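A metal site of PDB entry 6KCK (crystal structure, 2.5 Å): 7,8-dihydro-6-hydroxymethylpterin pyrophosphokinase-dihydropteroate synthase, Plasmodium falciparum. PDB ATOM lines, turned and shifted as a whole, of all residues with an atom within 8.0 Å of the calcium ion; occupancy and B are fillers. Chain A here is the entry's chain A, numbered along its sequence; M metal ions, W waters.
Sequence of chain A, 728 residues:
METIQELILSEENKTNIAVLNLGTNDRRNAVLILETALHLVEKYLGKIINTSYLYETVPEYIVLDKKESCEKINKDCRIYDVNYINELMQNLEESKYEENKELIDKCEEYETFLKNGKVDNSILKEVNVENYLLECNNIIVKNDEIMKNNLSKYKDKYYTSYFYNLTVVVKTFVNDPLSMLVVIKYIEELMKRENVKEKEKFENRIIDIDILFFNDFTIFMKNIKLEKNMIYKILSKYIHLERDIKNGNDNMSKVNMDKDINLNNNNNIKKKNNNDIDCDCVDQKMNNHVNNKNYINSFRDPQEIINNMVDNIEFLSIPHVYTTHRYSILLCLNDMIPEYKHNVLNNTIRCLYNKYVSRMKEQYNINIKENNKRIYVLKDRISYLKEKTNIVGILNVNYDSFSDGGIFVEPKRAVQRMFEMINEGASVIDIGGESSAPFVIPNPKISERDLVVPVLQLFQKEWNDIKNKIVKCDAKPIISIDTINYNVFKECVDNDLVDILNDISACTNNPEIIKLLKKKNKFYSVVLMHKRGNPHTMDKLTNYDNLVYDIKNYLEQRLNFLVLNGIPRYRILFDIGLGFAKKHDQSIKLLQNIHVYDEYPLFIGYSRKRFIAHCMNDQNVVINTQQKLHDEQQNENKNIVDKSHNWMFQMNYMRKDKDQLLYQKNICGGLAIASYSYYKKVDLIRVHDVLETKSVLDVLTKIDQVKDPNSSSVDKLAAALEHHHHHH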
ATOM      1  N   LEU A  38       0.559 -35.217   7.011  1.00  0.00           N
ATOM      2  CA  LEU A  38       1.423 -34.060   6.686  1.00  0.00           C
ATOM      3  C   LEU A  38       0.890 -32.812   7.312  1.00  0.00           C
ATOM      4  O   LEU A  38       1.648 -32.013   7.860  1.00  0.00           O
ATOM      5  CB  LEU A  38       1.585 -33.824   5.179  1.00  0.00           C
ATOM      6  CG  LEU A  38       2.526 -34.716   4.389  1.00  0.00           C
ATOM      7  CD1 LEU A  38       2.645 -34.214   2.971  1.00  0.00           C
ATOM      8  CD2 LEU A  38       3.913 -34.785   5.021  1.00  0.00           C
ATOM      9  N   HIS A  39      -0.428 -32.619   7.237  1.00  0.00           N
ATOM     10  CA  HIS A  39      -1.040 -31.411   7.830  1.00  0.00           C
ATOM     11  C   HIS A  39      -0.833 -31.385   9.319  1.00  0.00           C
ATOM     12  O   HIS A  39      -0.504 -30.361   9.878  1.00  0.00           O
ATOM     13  CB  HIS A  39      -2.527 -31.307   7.513  1.00  0.00           C
ATOM     14  CG  HIS A  39      -2.848 -31.041   6.062  1.00  0.00           C
ATOM     15  ND1 HIS A  39      -2.474 -29.919   5.419  1.00  0.00           N
ATOM     16  CD2 HIS A  39      -3.598 -31.789   5.137  1.00  0.00           C
ATOM     17  CE1 HIS A  39      -2.921 -29.953   4.149  1.00  0.00           C
ATOM     18  NE2 HIS A  39      -3.607 -31.102   3.977  1.00  0.00           N
ATOM     19  N   LEU A  40      -1.003 -32.530   9.964  1.00  0.00           N
ATOM     20  CA  LEU A  40      -0.938 -32.564  11.414  1.00  0.00           C
ATOM     21  C   LEU A  40       0.498 -32.444  11.854  1.00  0.00           C
ATOM     22  O   LEU A  40       0.784 -31.793  12.855  1.00  0.00           O
ATOM     23  CB  LEU A  40      -1.612 -33.811  11.967  1.00  0.00           C
ATOM     24  CG  LEU A  40      -3.119 -33.767  11.650  1.00  0.00           C
ATOM     25  CD1 LEU A  40      -3.835 -35.003  12.155  1.00  0.00           C
ATOM     26  CD2 LEU A  40      -3.778 -32.507  12.165  1.00  0.00           C
ATOM     27  N   VAL A  41       1.413 -33.016  11.067  1.00  0.00           N
ATOM     28  CA  VAL A  41       2.830 -32.757  11.274  1.00  0.00           C
ATOM     29  C   VAL A  41       3.150 -31.269  11.257  1.00  0.00           C
ATOM     30  O   VAL A  41       3.830 -30.777  12.157  1.00  0.00           O
ATOM     31  CB  VAL A  41       3.734 -33.510  10.288  1.00  0.00           C
ATOM     32  CG1 VAL A  41       5.166 -33.026  10.408  1.00  0.00           C
ATOM     33  CG2 VAL A  41       3.655 -34.999  10.559  1.00  0.00           C
ATOM     34  N   GLU A  42       2.637 -30.551  10.260  1.00  0.00           N
ATOM     35  CA  GLU A  42       2.945 -29.116  10.082  1.00  0.00           C
ATOM     36  C   GLU A  42       2.273 -28.307  11.174  1.00  0.00           C
ATOM     37  O   GLU A  42       2.730 -27.212  11.540  1.00  0.00           O
ATOM     38  CB  GLU A  42       2.497 -28.654   8.678  1.00  0.00           C
ATOM     39  CG  GLU A  42       2.645 -27.176   8.340  1.00  0.00           C
ATOM     40  CD  GLU A  42       4.080 -26.708   8.030  1.00  0.00           C
ATOM     41  OE1 GLU A  42       4.781 -27.277   7.137  1.00  0.00           O
ATOM     42  OE2 GLU A  42       4.516 -25.713   8.660  1.00  0.00           O
ATOM     43  N   LYS A  43       1.186 -28.840  11.720  1.00  0.00           N
ATOM     44  CA  LYS A  43       0.460 -28.105  12.739  1.00  0.00           C
ATOM     45  C   LYS A  43       1.077 -28.352  14.113  1.00  0.00           C
ATOM     46  O   LYS A  43       1.329 -27.419  14.868  1.00  0.00           O
ATOM     47  CB  LYS A  43      -0.993 -28.530  12.714  1.00  0.00           C
ATOM     48  CG  LYS A  43      -1.949 -27.797  13.652  1.00  0.00           C
ATOM     49  CD  LYS A  43      -3.356 -28.390  13.464  1.00  0.00           C
ATOM     50  CE  LYS A  43      -4.431 -27.704  14.308  1.00  0.00           C
ATOM     51  NZ  LYS A  43      -4.532 -26.227  14.102  1.00  0.00           N
ATOM     52  N   TYR A  44       1.315 -29.622  14.433  1.00  0.00           N
ATOM     53  CA  TYR A  44       1.672 -29.988  15.778  1.00  0.00           C
ATOM     54  C   TYR A  44       3.175 -30.150  16.032  1.00  0.00           C
ATOM     55  O   TYR A  44       3.574 -30.208  17.181  1.00  0.00           O
ATOM     56  CB  TYR A  44       0.927 -31.254  16.188  1.00  0.00           C
ATOM     57  CG  TYR A  44      -0.567 -31.080  16.406  1.00  0.00           C
ATOM     58  CD1 TYR A  44      -1.077 -29.976  17.075  1.00  0.00           C
ATOM     59  CD2 TYR A  44      -1.472 -32.047  15.960  1.00  0.00           C
ATOM     60  CE1 TYR A  44      -2.434 -29.823  17.289  1.00  0.00           C
ATOM     61  CE2 TYR A  44      -2.842 -31.919  16.160  1.00  0.00           C
ATOM     62  CZ  TYR A  44      -3.323 -30.808  16.825  1.00  0.00           C
ATOM     63  OH  TYR A  44      -4.692 -30.671  17.028  1.00  0.00           O
ATOM     64  N   LEU A  45       4.013 -30.186  14.990  1.00  0.00           N
ATOM     65  CA  LEU A  45       5.445 -30.454  15.179  1.00  0.00           C
ATOM     66  C   LEU A  45       6.446 -29.403  14.713  1.00  0.00           C
ATOM     67  O   LEU A  45       7.570 -29.369  15.217  1.00  0.00           O
ATOM     68  CB  LEU A  45       5.828 -31.811  14.569  1.00  0.00           C
ATOM     69  CG  LEU A  45       5.154 -33.058  15.122  1.00  0.00           C
ATOM     70  CD1 LEU A  45       5.629 -34.276  14.360  1.00  0.00           C
ATOM     71  CD2 LEU A  45       5.441 -33.223  16.609  1.00  0.00           C
ATOM     72  N   GLY A  46       6.095 -28.581  13.742  1.00  0.00           N
ATOM     73  CA  GLY A  46       7.039 -27.548  13.261  1.00  0.00           C
ATOM     74  C   GLY A  46       6.881 -27.318  11.772  1.00  0.00           C
ATOM     75  O   GLY A  46       5.789 -27.275  11.279  1.00  0.00           O
ATOM     76  N   LYS A  47       7.975 -27.184  11.040  1.00  0.00           N
ATOM     77  CA  LYS A  47       7.852 -26.866   9.626  1.00  0.00           C
ATOM     78  C   LYS A  47       8.446 -27.934   8.694  1.00  0.00           C
ATOM     79  O   LYS A  47       9.614 -28.293   8.834  1.00  0.00           O
ATOM     80  CB  LYS A  47       8.476 -25.489   9.332  1.00  0.00           C
ATOM     81  CG  LYS A  47       8.390 -25.099   7.872  1.00  0.00           C
ATOM     82  CD  LYS A  47       9.209 -23.855   7.598  1.00  0.00           C
ATOM     83  CE  LYS A  47       8.903 -23.276   6.221  1.00  0.00           C
ATOM     84  NZ  LYS A  47       7.421 -23.148   5.996  1.00  0.00           N
ATOM     85  N   ILE A  48       7.643 -28.413   7.745  1.00  0.00           N
ATOM     86  CA  ILE A  48       8.082 -29.326   6.667  1.00  0.00           C
ATOM     87  C   ILE A  48       8.992 -28.595   5.674  1.00  0.00           C
ATOM     88  O   ILE A  48       8.604 -27.593   5.099  1.00  0.00           O
ATOM     89  CB  ILE A  48       6.841 -29.932   5.948  1.00  0.00           C
ATOM     90  CG1 ILE A  48       5.907 -30.576   7.016  1.00  0.00           C
ATOM     91  CG2 ILE A  48       7.273 -30.916   4.862  1.00  0.00           C
ATOM     92  CD1 ILE A  48       4.818 -31.512   6.535  1.00  0.00           C
ATOM     93  N   SER A  95      -2.550 -25.410  18.143  1.00  0.00           N
ATOM     94  CA  SER A  95      -1.193 -25.675  18.537  1.00  0.00           C
ATOM     95  C   SER A  95      -0.772 -24.491  19.352  1.00  0.00           C
ATOM     96  O   SER A  95      -1.138 -23.359  19.031  1.00  0.00           O
ATOM     97  CB  SER A  95      -0.274 -25.835  17.338  1.00  0.00           C
ATOM     98  OG  SER A  95       1.098 -25.774  17.727  1.00  0.00           O
ATOM     99  N   TYR A  97       2.000 -23.510  19.289  1.00  0.00           N
ATOM    100  CA  TYR A  97       3.104 -22.924  18.527  1.00  0.00           C
ATOM    101  C   TYR A  97       2.662 -22.308  17.206  1.00  0.00           C
ATOM    102  O   TYR A  97       1.686 -22.751  16.576  1.00  0.00           O
ATOM    103  CB  TYR A  97       4.189 -23.956  18.284  1.00  0.00           C
ATOM    104  CG  TYR A  97       5.164 -24.124  19.417  1.00  0.00           C
ATOM    105  CD1 TYR A  97       4.828 -24.898  20.526  1.00  0.00           C
ATOM    106  CD2 TYR A  97       6.426 -23.530  19.373  1.00  0.00           C
ATOM    107  CE1 TYR A  97       5.739 -25.041  21.577  1.00  0.00           C
ATOM    108  CE2 TYR A  97       7.331 -23.677  20.408  1.00  0.00           C
ATOM    109  CZ  TYR A  97       6.977 -24.432  21.498  1.00  0.00           C
ATOM    110  OH  TYR A  97       7.867 -24.611  22.541  1.00  0.00           O
ATOM    111  N   GLU A  98       3.418 -21.298  16.796  1.00  0.00           N
ATOM    112  CA  GLU A  98       3.133 -20.499  15.623  1.00  0.00           C
ATOM    113  C   GLU A  98       3.255 -21.245  14.338  1.00  0.00           C
ATOM    114  O   GLU A  98       4.096 -22.136  14.213  1.00  0.00           O
ATOM    115  CB  GLU A  98       4.116 -19.373  15.542  1.00  0.00           C
ATOM    116  CG  GLU A  98       3.756 -18.240  16.453  1.00  0.00           C
ATOM    117  CD  GLU A  98       4.769 -17.147  16.361  1.00  0.00           C
ATOM    118  OE1 GLU A  98       5.918 -17.423  15.934  1.00  0.00           O
ATOM    119  OE2 GLU A  98       4.386 -16.007  16.710  1.00  0.00           O
ATOM    120  N   GLU A  99       2.412 -20.846  13.382  1.00  0.00           N
ATOM    121  CA  GLU A  99       2.533 -21.199  11.988  1.00  0.00           C
ATOM    122  C   GLU A  99       2.990 -19.965  11.216  1.00  0.00           C
ATOM    123  O   GLU A  99       2.319 -18.925  11.249  1.00  0.00           O
ATOM    124  CB  GLU A  99       1.182 -21.658  11.470  1.00  0.00           C
ATOM    125  CG  GLU A  99       1.230 -22.340  10.118  1.00  0.00           C
ATOM    126  CD  GLU A  99       2.189 -23.503  10.092  1.00  0.00           C
ATOM    127  OE1 GLU A  99       1.769 -24.588  10.537  1.00  0.00           O
ATOM    128  OE2 GLU A  99       3.353 -23.322   9.652  1.00  0.00           O
ATOM    129  N   ASN A 100       4.141 -20.034  10.560  1.00  0.00           N
ATOM    130  CA  ASN A 100       4.601 -18.930   9.727  1.00  0.00           C
ATOM    131  C   ASN A 100       4.712 -19.365   8.299  1.00  0.00           C
ATOM    132  O   ASN A 100       5.561 -20.197   7.977  1.00  0.00           O
ATOM    133  CB  ASN A 100       5.937 -18.379  10.196  1.00  0.00           C
ATOM    134  CG  ASN A 100       5.847 -17.751  11.570  1.00  0.00           C
ATOM    135  OD1 ASN A 100       4.991 -16.913  11.842  1.00  0.00           O
ATOM    136  ND2 ASN A 100       6.772 -18.129  12.451  1.00  0.00           N
ATOM    137  N   LYS A 101       3.858 -18.805   7.441  1.00  0.00           N
ATOM    138  CA  LYS A 101       3.853 -19.150   6.020  1.00  0.00           C
ATOM    139  C   LYS A 101       4.823 -18.356   5.172  1.00  0.00           C
ATOM    140  O   LYS A 101       5.000 -18.676   4.022  1.00  0.00           O
ATOM    141  CB  LYS A 101       2.432 -19.083   5.450  1.00  0.00           C
ATOM    142  CG  LYS A 101       1.472 -20.028   6.165  1.00  0.00           C
ATOM    143  CD  LYS A 101       0.021 -19.897   5.710  1.00  0.00           C
ATOM    144  CE  LYS A 101      -0.904 -20.524   6.751  1.00  0.00           C
ATOM    145  NZ  LYS A 101      -2.379 -20.364   6.489  1.00  0.00           N
ATOM    146  N   VAL A 170      11.445 -32.289   9.129  1.00  0.00           N
ATOM    147  CA  VAL A 170      10.694 -31.281   9.857  1.00  0.00           C
ATOM    148  C   VAL A 170      11.662 -30.473  10.679  1.00  0.00           C
ATOM    149  O   VAL A 170      12.476 -31.035  11.392  1.00  0.00           O
ATOM    150  CB  VAL A 170       9.665 -31.920  10.820  1.00  0.00           C
ATOM    151  CG1 VAL A 170       8.674 -30.872  11.339  1.00  0.00           C
ATOM    152  CG2 VAL A 170       8.916 -33.060  10.135  1.00  0.00           C
ATOM    153  N   LYS A 171      11.603 -29.159  10.536  1.00  0.00           N
ATOM    154  CA  LYS A 171      12.290 -28.254  11.432  1.00  0.00           C
ATOM    155  C   LYS A 171      11.388 -28.156  12.651  1.00  0.00           C
ATOM    156  O   LYS A 171      10.364 -27.463  12.622  1.00  0.00           O
ATOM    157  CB  LYS A 171      12.509 -26.902  10.778  1.00  0.00           C
ATOM    158  CG  LYS A 171      13.064 -25.862  11.716  1.00  0.00           C
ATOM    159  CD  LYS A 171      14.015 -24.915  10.996  1.00  0.00           C
ATOM    160  CE  LYS A 171      13.288 -23.880  10.148  1.00  0.00           C
ATOM    161  NZ  LYS A 171      14.284 -23.106   9.348  1.00  0.00           N
ATOM    162  N   PHE A 173      10.064 -27.801  16.763  1.00  0.00           N
ATOM    163  CA  PHE A 173      10.190 -27.028  18.002  1.00  0.00           C
ATOM    164  C   PHE A 173      10.048 -27.923  19.228  1.00  0.00           C
ATOM    165  O   PHE A 173      10.025 -27.453  20.361  1.00  0.00           O
ATOM    166  CB  PHE A 173       9.191 -25.862  18.040  1.00  0.00           C
ATOM    167  CG  PHE A 173       7.794 -26.231  17.596  1.00  0.00           C
ATOM    168  CD1 PHE A 173       7.036 -27.171  18.293  1.00  0.00           C
ATOM    169  CD2 PHE A 173       7.215 -25.594  16.518  1.00  0.00           C
ATOM    170  CE1 PHE A 173       5.760 -27.489  17.898  1.00  0.00           C
ATOM    171  CE2 PHE A 173       5.936 -25.908  16.110  1.00  0.00           C
ATOM    172  CZ  PHE A 173       5.209 -26.857  16.788  1.00  0.00           C
ATOM    173  N   LYS A 518      -1.017 -24.445  -0.428  1.00  0.00           N
ATOM    174  CA  LYS A 518      -1.343 -25.164   0.806  1.00  0.00           C
ATOM    175  C   LYS A 518      -2.540 -24.537   1.491  1.00  0.00           C
ATOM    176  O   LYS A 518      -2.645 -23.311   1.553  1.00  0.00           O
ATOM    177  CB  LYS A 518      -0.169 -25.135   1.781  1.00  0.00           C
ATOM    178  CG  LYS A 518       1.144 -25.616   1.209  1.00  0.00           C
ATOM    179  CD  LYS A 518       2.330 -24.835   1.765  1.00  0.00           C
ATOM    180  CE  LYS A 518       2.887 -25.487   3.006  1.00  0.00           C
ATOM    181  NZ  LYS A 518       4.184 -24.863   3.394  1.00  0.00           N
HETATM  182 CA    CA M   1       4.092 -25.404  11.109  1.00  0.00          CA
HETATM  183  O   HOH W   1       5.869 -24.150  11.125  1.00  0.00           O
HETATM  184  O   HOH W   2       2.771 -24.692  13.820  1.00  0.00           O
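The side-chain carboxylate (OE1) of Glu 42 is in hydrogen-bond range of the backbone NH (N) of Ile 48 (3.1 Å).
Water W2 bridges O of Glu 98 (2.9 Å) and O of Lys 43 (3.3 Å).
Within 4 Å of the calcium ion: Glu 42, Gly 46 and Glu 99.
The calcium ion is bound by water W1 (2.2 Å), O of Glu 42 (2.3 Å), OE2 of Glu 42 (2.5 Å), OE1 of Glu 99 (2.5 Å), O of Gly 46 (2.5 Å) and OE2 of Glu 99 (2.6 Å).
Slightly farther from the calcium ion lies water W2 (3.1 Å).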
